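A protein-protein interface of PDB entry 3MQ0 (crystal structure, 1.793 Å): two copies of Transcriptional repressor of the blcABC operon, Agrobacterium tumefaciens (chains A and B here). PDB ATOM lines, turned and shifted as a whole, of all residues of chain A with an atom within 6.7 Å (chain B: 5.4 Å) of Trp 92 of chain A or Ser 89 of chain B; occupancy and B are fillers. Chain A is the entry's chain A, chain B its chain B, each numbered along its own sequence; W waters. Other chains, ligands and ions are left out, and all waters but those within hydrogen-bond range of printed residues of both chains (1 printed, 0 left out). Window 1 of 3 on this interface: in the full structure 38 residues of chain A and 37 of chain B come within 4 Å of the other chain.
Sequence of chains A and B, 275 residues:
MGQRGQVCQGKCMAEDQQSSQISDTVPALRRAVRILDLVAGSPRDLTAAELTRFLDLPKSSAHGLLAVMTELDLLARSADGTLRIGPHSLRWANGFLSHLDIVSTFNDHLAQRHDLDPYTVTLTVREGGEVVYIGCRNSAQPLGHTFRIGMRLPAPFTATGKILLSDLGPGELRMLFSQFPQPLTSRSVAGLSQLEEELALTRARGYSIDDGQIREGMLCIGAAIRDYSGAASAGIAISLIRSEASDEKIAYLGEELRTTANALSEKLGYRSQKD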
ATOM      1  N   LEU A  36       0.961   6.501  23.730  1.00  0.00           N
ATOM      2  CA  LEU A  36       1.908   7.305  22.984  1.00  0.00           C
ATOM      3  C   LEU A  36       2.067   8.697  23.590  1.00  0.00           C
ATOM      4  O   LEU A  36       3.186   9.223  23.667  1.00  0.00           O
ATOM      5  CB  LEU A  36       1.510   7.392  21.513  1.00  0.00           C
ATOM      6  CG  LEU A  36       1.637   6.074  20.770  1.00  0.00           C
ATOM      7  CD1 LEU A  36       0.987   6.219  19.372  1.00  0.00           C
ATOM      8  CD2 LEU A  36       3.111   5.664  20.660  1.00  0.00           C
ATOM      9  N   LEU A  74       5.610   1.413  16.735  1.00  0.00           N
ATOM     10  CA  LEU A  74       5.046   2.593  17.389  1.00  0.00           C
ATOM     11  C   LEU A  74       5.804   2.869  18.683  1.00  0.00           C
ATOM     12  O   LEU A  74       6.001   4.024  19.072  1.00  0.00           O
ATOM     13  CB  LEU A  74       3.558   2.383  17.691  1.00  0.00           C
ATOM     14  CG  LEU A  74       2.617   2.235  16.490  1.00  0.00           C
ATOM     15  CD1 LEU A  74       1.143   2.192  16.926  1.00  0.00           C
ATOM     16  CD2 LEU A  74       2.856   3.370  15.533  1.00  0.00           C
ATOM     17  N   PRO A  87      10.191   4.569  15.741  1.00  0.00           N
ATOM     18  CA  PRO A  87      10.379   5.407  14.547  1.00  0.00           C
ATOM     19  C   PRO A  87       9.129   5.593  13.687  1.00  0.00           C
ATOM     20  O   PRO A  87       9.082   6.549  12.910  1.00  0.00           O
ATOM     21  CB  PRO A  87      11.462   4.651  13.752  1.00  0.00           C
ATOM     22  CG  PRO A  87      11.354   3.240  14.204  1.00  0.00           C
ATOM     23  CD  PRO A  87      10.909   3.283  15.647  1.00  0.00           C
ATOM     24  N   HIS A  88       8.146   4.709  13.817  1.00  0.00           N
ATOM     25  CA  HIS A  88       6.970   4.760  12.944  1.00  0.00           C
ATOM     26  C   HIS A  88       6.293   6.141  12.893  1.00  0.00           C
ATOM     27  O   HIS A  88       5.948   6.625  11.812  1.00  0.00           O
ATOM     28  CB  HIS A  88       5.954   3.687  13.340  1.00  0.00           C
ATOM     29  CG  HIS A  88       5.074   3.251  12.213  1.00  0.00           C
ATOM     30  ND1 HIS A  88       4.903   1.928  11.875  1.00  0.00           N
ATOM     31  CD2 HIS A  88       4.334   3.964  11.336  1.00  0.00           C
ATOM     32  CE1 HIS A  88       4.083   1.842  10.839  1.00  0.00           C
ATOM     33  NE2 HIS A  88       3.737   3.067  10.486  1.00  0.00           N
ATOM     34  N   SER A  89       6.098   6.764  14.052  1.00  0.00           N
ATOM     35  CA  SER A  89       5.416   8.065  14.146  1.00  0.00           C
ATOM     36  C   SER A  89       6.028   9.126  13.245  1.00  0.00           C
ATOM     37  O   SER A  89       5.342  10.011  12.739  1.00  0.00           O
ATOM     38  CB  SER A  89       5.466   8.577  15.592  1.00  0.00           C
ATOM     39  OG  SER A  89       4.471   7.959  16.367  1.00  0.00           O
ATOM     40  N   LEU A  90       7.337   9.047  13.072  1.00  0.00           N
ATOM     41  CA  LEU A  90       8.079  10.015  12.280  1.00  0.00           C
ATOM     42  C   LEU A  90       7.605   9.972  10.826  1.00  0.00           C
ATOM     43  O   LEU A  90       7.591  10.989  10.143  1.00  0.00           O
ATOM     44  CB  LEU A  90       9.570   9.678  12.356  1.00  0.00           C
ATOM     45  CG  LEU A  90      10.573  10.749  11.939  1.00  0.00           C
ATOM     46  CD1 LEU A  90      10.274  12.055  12.637  1.00  0.00           C
ATOM     47  CD2 LEU A  90      11.991  10.284  12.251  1.00  0.00           C
ATOM     48  N   ARG A  91       7.219   8.788  10.362  1.00  0.00           N
ATOM     49  CA  ARG A  91       6.649   8.621   9.027  1.00  0.00           C
ATOM     50  C   ARG A  91       5.344   9.406   8.860  1.00  0.00           C
ATOM     51  O   ARG A  91       5.087   9.985   7.802  1.00  0.00           O
ATOM     52  CB  ARG A  91       6.365   7.146   8.745  1.00  0.00           C
ATOM     53  CG  ARG A  91       7.601   6.262   8.689  1.00  0.00           C
ATOM     54  CD  ARG A  91       7.202   4.817   8.447  1.00  0.00           C
ATOM     55  NE  ARG A  91       6.328   4.690   7.281  1.00  0.00           N
ATOM     56  CZ  ARG A  91       5.797   3.544   6.867  1.00  0.00           C
ATOM     57  NH1 ARG A  91       6.052   2.421   7.528  1.00  0.00           N
ATOM     58  NH2 ARG A  91       5.014   3.518   5.792  1.00  0.00           N
ATOM     59  N   TRP A  92       4.516   9.410   9.898  1.00  0.00           N
ATOM     60  CA  TRP A  92       3.262  10.155   9.849  1.00  0.00           C
ATOM     61  C   TRP A  92       3.525  11.651   9.922  1.00  0.00           C
ATOM     62  O   TRP A  92       2.872  12.441   9.225  1.00  0.00           O
ATOM     63  CB  TRP A  92       2.346   9.733  10.992  1.00  0.00           C
ATOM     64  CG  TRP A  92       2.031   8.282  10.955  1.00  0.00           C
ATOM     65  CD1 TRP A  92       2.069   7.465   9.858  1.00  0.00           C
ATOM     66  CD2 TRP A  92       1.630   7.463  12.055  1.00  0.00           C
ATOM     67  NE1 TRP A  92       1.719   6.190  10.214  1.00  0.00           N
ATOM     68  CE2 TRP A  92       1.442   6.160  11.555  1.00  0.00           C
ATOM     69  CE3 TRP A  92       1.417   7.703  13.422  1.00  0.00           C
ATOM     70  CZ2 TRP A  92       1.053   5.102  12.365  1.00  0.00           C
ATOM     71  CZ3 TRP A  92       1.023   6.649  14.224  1.00  0.00           C
ATOM     72  CH2 TRP A  92       0.843   5.365  13.693  1.00  0.00           C
ATOM     73  N   ALA A  93       4.452  12.045  10.788  1.00  0.00           N
ATOM     74  CA  ALA A  93       4.819  13.455  10.910  1.00  0.00           C
ATOM     75  C   ALA A  93       5.429  13.986   9.620  1.00  0.00           C
ATOM     76  O   ALA A  93       5.171  15.125   9.236  1.00  0.00           O
ATOM     77  CB  ALA A  93       5.771  13.666  12.072  1.00  0.00           C
ATOM     78  N   ASN A  94       6.257  13.181   8.958  1.00  0.00           N
ATOM     79  CA  ASN A  94       6.798  13.598   7.671  1.00  0.00           C
ATOM     80  C   ASN A  94       5.710  13.729   6.614  1.00  0.00           C
ATOM     81  O   ASN A  94       5.765  14.620   5.765  1.00  0.00           O
ATOM     82  CB  ASN A  94       7.879  12.641   7.181  1.00  0.00           C
ATOM     83  CG  ASN A  94       9.195  12.836   7.905  1.00  0.00           C
ATOM     84  OD1 ASN A  94       9.486  13.924   8.397  1.00  0.00           O
ATOM     85  ND2 ASN A  94      10.004  11.779   7.967  1.00  0.00           N
ATOM     86  N   GLY A  95       4.720  12.842   6.672  1.00  0.00           N
ATOM     87  CA  GLY A  95       3.610  12.896   5.732  1.00  0.00           C
ATOM     88  C   GLY A  95       2.798  14.157   5.994  1.00  0.00           C
ATOM     89  O   GLY A  95       2.362  14.834   5.065  1.00  0.00           O
ATOM     90  N   PHE A  96       2.620  14.486   7.264  1.00  0.00           N
ATOM     91  CA  PHE A  96       1.945  15.734   7.641  1.00  0.00           C
ATOM     92  C   PHE A  96       2.656  16.954   7.029  1.00  0.00           C
ATOM     93  O   PHE A  96       2.036  17.792   6.362  1.00  0.00           O
ATOM     94  CB  PHE A  96       1.874  15.869   9.176  1.00  0.00           C
ATOM     95  CG  PHE A  96       1.237  17.154   9.642  1.00  0.00           C
ATOM     96  CD1 PHE A  96      -0.131  17.248   9.793  1.00  0.00           C
ATOM     97  CD2 PHE A  96       2.013  18.273   9.904  1.00  0.00           C
ATOM     98  CE1 PHE A  96      -0.725  18.438  10.222  1.00  0.00           C
ATOM     99  CE2 PHE A  96       1.430  19.467  10.317  1.00  0.00           C
ATOM    100  CZ  PHE A  96       0.050  19.542  10.475  1.00  0.00           C
ATOM    101  N   LEU A  97       3.961  17.037   7.246  1.00  0.00           N
ATOM    102  CA  LEU A  97       4.718  18.206   6.831  1.00  0.00           C
ATOM    103  C   LEU A  97       4.822  18.309   5.316  1.00  0.00           C
ATOM    104  O   LEU A  97       4.775  19.404   4.766  1.00  0.00           O
ATOM    105  CB  LEU A  97       6.098  18.210   7.490  1.00  0.00           C
ATOM    106  CG  LEU A  97       6.025  18.396   9.005  1.00  0.00           C
ATOM    107  CD1 LEU A  97       7.392  18.204   9.656  1.00  0.00           C
ATOM    108  CD2 LEU A  97       5.442  19.768   9.330  1.00  0.00           C
ATOM    109  N   VAL B  33      -3.223   1.830  11.688  1.00  0.00           N
ATOM    110  CA  VAL B  33      -1.841   2.007  11.251  1.00  0.00           C
ATOM    111  C   VAL B  33      -1.717   1.900   9.723  1.00  0.00           C
ATOM    112  O   VAL B  33      -1.038   2.710   9.083  1.00  0.00           O
ATOM    113  CB  VAL B  33      -0.912   1.034  11.975  1.00  0.00           C
ATOM    114  CG1 VAL B  33       0.495   1.060  11.365  1.00  0.00           C
ATOM    115  CG2 VAL B  33      -0.873   1.397  13.463  1.00  0.00           C
ATOM    116  N   LEU B  36      -3.061   5.189   8.316  1.00  0.00           N
ATOM    117  CA  LEU B  36      -2.124   6.293   8.483  1.00  0.00           C
ATOM    118  C   LEU B  36      -0.949   6.177   7.522  1.00  0.00           C
ATOM    119  O   LEU B  36      -0.502   7.178   6.958  1.00  0.00           O
ATOM    120  CB  LEU B  36      -1.649   6.416   9.932  1.00  0.00           C
ATOM    121  CG  LEU B  36      -2.790   6.888  10.846  1.00  0.00           C
ATOM    122  CD1 LEU B  36      -2.475   6.555  12.289  1.00  0.00           C
ATOM    123  CD2 LEU B  36      -3.080   8.382  10.697  1.00  0.00           C
ATOM    124  N   ASP B  37      -0.458   4.962   7.310  1.00  0.00           N
ATOM    125  CA  ASP B  37       0.634   4.790   6.360  1.00  0.00           C
ATOM    126  C   ASP B  37       0.222   5.199   4.944  1.00  0.00           C
ATOM    127  O   ASP B  37       1.008   5.800   4.215  1.00  0.00           O
ATOM    128  CB  ASP B  37       1.145   3.357   6.368  1.00  0.00           C
ATOM    129  CG  ASP B  37       1.933   3.019   7.625  1.00  0.00           C
ATOM    130  OD1 ASP B  37       2.297   3.937   8.406  1.00  0.00           O
ATOM    131  OD2 ASP B  37       2.204   1.820   7.822  1.00  0.00           O
ATOM    132  N   ALA B  40      -0.107   9.008   4.755  1.00  0.00           N
ATOM    133  CA  ALA B  40       1.178   9.664   4.852  1.00  0.00           C
ATOM    134  C   ALA B  40       1.938   9.549   3.541  1.00  0.00           C
ATOM    135  O   ALA B  40       2.669  10.463   3.162  1.00  0.00           O
ATOM    136  CB  ALA B  40       1.988   9.076   6.013  1.00  0.00           C
ATOM    137  N   LEU B  74      -6.215  11.474  14.939  1.00  0.00           N
ATOM    138  CA  LEU B  74      -5.192  10.832  14.122  1.00  0.00           C
ATOM    139  C   LEU B  74      -5.264  11.361  12.685  1.00  0.00           C
ATOM    140  O   LEU B  74      -4.236  11.552  12.035  1.00  0.00           O
ATOM    141  CB  LEU B  74      -5.377   9.313  14.133  1.00  0.00           C
ATOM    142  CG  LEU B  74      -5.229   8.677  15.520  1.00  0.00           C
ATOM    143  CD1 LEU B  74      -5.701   7.256  15.447  1.00  0.00           C
ATOM    144  CD2 LEU B  74      -3.772   8.760  15.990  1.00  0.00           C
ATOM    145  N   ILE B  85      -3.204  13.485   7.544  1.00  0.00           N
ATOM    146  CA  ILE B  85      -2.657  13.232   8.866  1.00  0.00           C
ATOM    147  C   ILE B  85      -2.970  14.400   9.803  1.00  0.00           C
ATOM    148  O   ILE B  85      -2.791  15.564   9.431  1.00  0.00           O
ATOM    149  CB  ILE B  85      -1.129  13.050   8.807  1.00  0.00           C
ATOM    150  CG1 ILE B  85      -0.762  11.894   7.866  1.00  0.00           C
ATOM    151  CG2 ILE B  85      -0.565  12.823  10.210  1.00  0.00           C
ATOM    152  CD1 ILE B  85      -1.230  10.531   8.346  1.00  0.00           C
ATOM    153  N   GLY B  86      -3.400  14.084  11.023  1.00  0.00           N
ATOM    154  CA  GLY B  86      -3.641  15.090  12.043  1.00  0.00           C
ATOM    155  C   GLY B  86      -2.327  15.569  12.631  1.00  0.00           C
ATOM    156  O   GLY B  86      -1.360  14.818  12.666  1.00  0.00           O
ATOM    157  N   PRO B  87      -2.279  16.828  13.077  1.00  0.00           N
ATOM    158  CA  PRO B  87      -1.044  17.442  13.583  1.00  0.00           C
ATOM    159  C   PRO B  87      -0.551  16.818  14.883  1.00  0.00           C
ATOM    160  O   PRO B  87       0.592  17.046  15.274  1.00  0.00           O
ATOM    161  CB  PRO B  87      -1.447  18.891  13.827  1.00  0.00           C
ATOM    162  CG  PRO B  87      -2.942  18.859  13.939  1.00  0.00           C
ATOM    163  CD  PRO B  87      -3.394  17.785  13.024  1.00  0.00           C
ATOM    164  N   HIS B  88      -1.399  16.046  15.548  1.00  0.00           N
ATOM    165  CA  HIS B  88      -1.014  15.482  16.839  1.00  0.00           C
ATOM    166  C   HIS B  88       0.172  14.522  16.719  1.00  0.00           C
ATOM    167  O   HIS B  88       0.929  14.342  17.677  1.00  0.00           O
ATOM    168  CB  HIS B  88      -2.199  14.773  17.497  1.00  0.00           C
ATOM    169  CG  HIS B  88      -1.962  14.403  18.927  1.00  0.00           C
ATOM    170  ND1 HIS B  88      -1.984  15.329  19.949  1.00  0.00           N
ATOM    171  CD2 HIS B  88      -1.694  13.208  19.506  1.00  0.00           C
ATOM    172  CE1 HIS B  88      -1.738  14.719  21.098  1.00  0.00           C
ATOM    173  NE2 HIS B  88      -1.559  13.431  20.854  1.00  0.00           N
ATOM    174  N   SER B  89       0.329  13.906  15.548  1.00  0.00           N
ATOM    175  CA  SER B  89       1.451  13.005  15.297  1.00  0.00           C
ATOM    176  C   SER B  89       2.786  13.687  15.512  1.00  0.00           C
ATOM    177  O   SER B  89       3.783  13.035  15.844  1.00  0.00           O
ATOM    178  CB  SER B  89       1.385  12.444  13.875  1.00  0.00           C
ATOM    179  OG  SER B  89       0.716  11.202  13.874  1.00  0.00           O
ATOM    180  N   LEU B  90       2.822  14.996  15.306  1.00  0.00           N
ATOM    181  CA  LEU B  90       4.058  15.739  15.516  1.00  0.00           C
ATOM    182  C   LEU B  90       4.566  15.582  16.954  1.00  0.00           C
ATOM    183  O   LEU B  90       5.777  15.567  17.191  1.00  0.00           O
ATOM    184  CB  LEU B  90       3.869  17.223  15.189  1.00  0.00           C
ATOM    185  CG  LEU B  90       3.625  17.558  13.714  1.00  0.00           C
ATOM    186  CD1 LEU B  90       3.392  19.056  13.533  1.00  0.00           C
ATOM    187  CD2 LEU B  90       4.781  17.097  12.861  1.00  0.00           C
ATOM    188  N   ARG B  91       3.642  15.474  17.909  1.00  0.00           N
ATOM    189  CA  ARG B  91       4.032  15.365  19.316  1.00  0.00           C
ATOM    190  C   ARG B  91       4.820  14.078  19.525  1.00  0.00           C
ATOM    191  O   ARG B  91       5.801  14.050  20.260  1.00  0.00           O
ATOM    192  CB  ARG B  91       2.798  15.403  20.234  1.00  0.00           C
ATOM    193  N   TRP B  92       4.388  13.009  18.876  1.00  0.00           N
ATOM    194  CA  TRP B  92       5.067  11.727  19.024  1.00  0.00           C
ATOM    195  C   TRP B  92       6.413  11.765  18.314  1.00  0.00           C
ATOM    196  O   TRP B  92       7.418  11.302  18.856  1.00  0.00           O
ATOM    197  CB  TRP B  92       4.189  10.611  18.471  1.00  0.00           C
ATOM    198  CG  TRP B  92       2.859  10.561  19.150  1.00  0.00           C
ATOM    199  CD1 TRP B  92       2.578  10.938  20.424  1.00  0.00           C
ATOM    200  CD2 TRP B  92       1.624  10.125  18.578  1.00  0.00           C
ATOM    201  NE1 TRP B  92       1.248  10.749  20.691  1.00  0.00           N
ATOM    202  CE2 TRP B  92       0.640  10.246  19.575  1.00  0.00           C
ATOM    203  CE3 TRP B  92       1.262   9.632  17.324  1.00  0.00           C
ATOM    204  CZ2 TRP B  92      -0.690   9.898  19.353  1.00  0.00           C
ATOM    205  CZ3 TRP B  92      -0.065   9.282  17.106  1.00  0.00           C
ATOM    206  CH2 TRP B  92      -1.020   9.416  18.112  1.00  0.00           C
ATOM    207  N   ALA B  93       6.442  12.313  17.101  1.00  0.00           N
ATOM    208  CA  ALA B  93       7.706  12.397  16.382  1.00  0.00           C
ATOM    209  C   ALA B  93       8.711  13.221  17.196  1.00  0.00           C
ATOM    210  O   ALA B  93       9.888  12.879  17.270  1.00  0.00           O
ATOM    211  CB  ALA B  93       7.500  12.995  14.974  1.00  0.00           C
ATOM    212  N   ASN B  94       8.233  14.300  17.817  1.00  0.00           N
ATOM    213  CA  ASN B  94       9.077  15.146  18.657  1.00  0.00           C
ATOM    214  C   ASN B  94       9.600  14.345  19.833  1.00  0.00           C
ATOM    215  O   ASN B  94      10.752  14.463  20.234  1.00  0.00           O
ATOM    216  CB  ASN B  94       8.259  16.338  19.164  1.00  0.00           C
ATOM    217  CG  ASN B  94       9.094  17.339  19.923  1.00  0.00           C
ATOM    218  OD1 ASN B  94       9.316  17.198  21.126  1.00  0.00           O
ATOM    219  ND2 ASN B  94       9.552  18.370  19.226  1.00  0.00           N
HETATM  220  O   HOH W   1       3.790   5.574   4.129  1.00  0.00           O
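NE1 of Trp 92 of chain A lies within hydrogen-bond range of OD1 of Asp 37 of chain B (2.9 Å). NE2 of His 88 of chain A lies within hydrogen-bond range of OD1 of Asp 37 of chain B (2.7 Å). The guanidinium group (NH2) of Arg 91 of chain A lies within salt-bridge range of the side-chain carboxylate (OD1) of Asp 37 of chain B, 3.8 Å away.
The backbone carbonyl oxygen (O) of Leu 90 of chain A lies close to the side-chain amide nitrogen (ND2) of Asn 94 of chain A, at 3.3 Å. O of Leu 74 of chain B is in hydrogen-bond range of N of Gly 86 of chain B (2.9 Å).
Among the printed residues, merely in contact across the chains: Leu 36 of chain A with Trp 92 of chain B (3.5 Å), His 88 of chain A with Val 33 of chain B (3.7 Å), Ser 89 of chain A with Trp 92 of chain B (3.4 Å), Leu 90 of chain A with Ala 93 of chain B (3.7 Å), Arg 91 of chain A with Ala 40 of chain B (3.7 Å), Trp 92 of chain A with Leu 36 of chain B (3.4 Å), Trp 92 of chain A with Ile 85 of chain B (3.6 Å), Trp 92 of chain A with Ser 89 of chain B (3.6 Å), Ala 93 of chain A with Leu 90 of chain B (3.7 Å), Ala 93 of chain A with Ala 93 of chain B (3.4 Å), Gly 95 of chain A with Ala 40 of chain B (3.7 Å), Phe 96 of chain A with Ile 85 of chain B (3.2 Å), Phe 96 of chain A with Gly 86 of chain B (3.96 Å), Phe 96 of chain A with Pro 87 of chain B (3.5 Å) and Phe 96 of chain A with Leu 90 of chain B (3.8 Å).
Of chain B, only Leu 36, Asp 37, Ile 85 and Ser 89 come within 4 Å of Trp 92 of chain A. Ser 89 of chain B touches one residue of chain A. Of the printed residues of chain A, Trp 92 of chain B touches Leu 36 and Ser 89. Of the printed residues of chain A, Leu 36 of chain B touches Trp 92. Of the printed residues of chain B, Ser 89 of chain A touches Trp 92. His 88 of chain B touches none of the printed residues of chain A. Asn 94 of chain A touches none of the printed residues of chain B. The nearest printed residue of chain A that does not touch Val 33 of chain B is Leu 74 of chain A (4.1 Å).
Of the 15 printed residues of chain B, 11 touch a printed residue of chain A. Hydrophobic or aromatic side chains of chain B that line the printed part of chain A: Val 33, Leu 36, Ala 40, Ile 85, Pro 87, Leu 90, Trp 92 and Ala 93. Hydrophobic or aromatic side chains of chain A that line the printed part of chain B: Leu 36, His 88, Leu 90, Trp 92, Ala 93 and Phe 96.
Leu 36 of chain A touches Trp 92 of chain B, and with the chains exchanged Trp 92 of chain A touches Leu 36 of chain B. Ser 89 of chain A touches Trp 92 of chain B, and with the chains exchanged Trp 92 of chain A touches Ser 89 of chain B. Leu 90 of chain A touches Ala 93 of chain B, and with the chains exchanged Ala 93 of chain A touches Leu 90 of chain B. Ala 93 of chain B touches its own counterpart, Ala 93 of chain A. Positions printed for both chains: 36, 74, 87, 88, 89, 90, 91, 92, 93 and 94.
Water W1 bridges the backbone carbonyl oxygen of Asp 37 of chain B (2.8 Å) and the guanidinium group of Arg 91 of chain A (2.9 Å).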
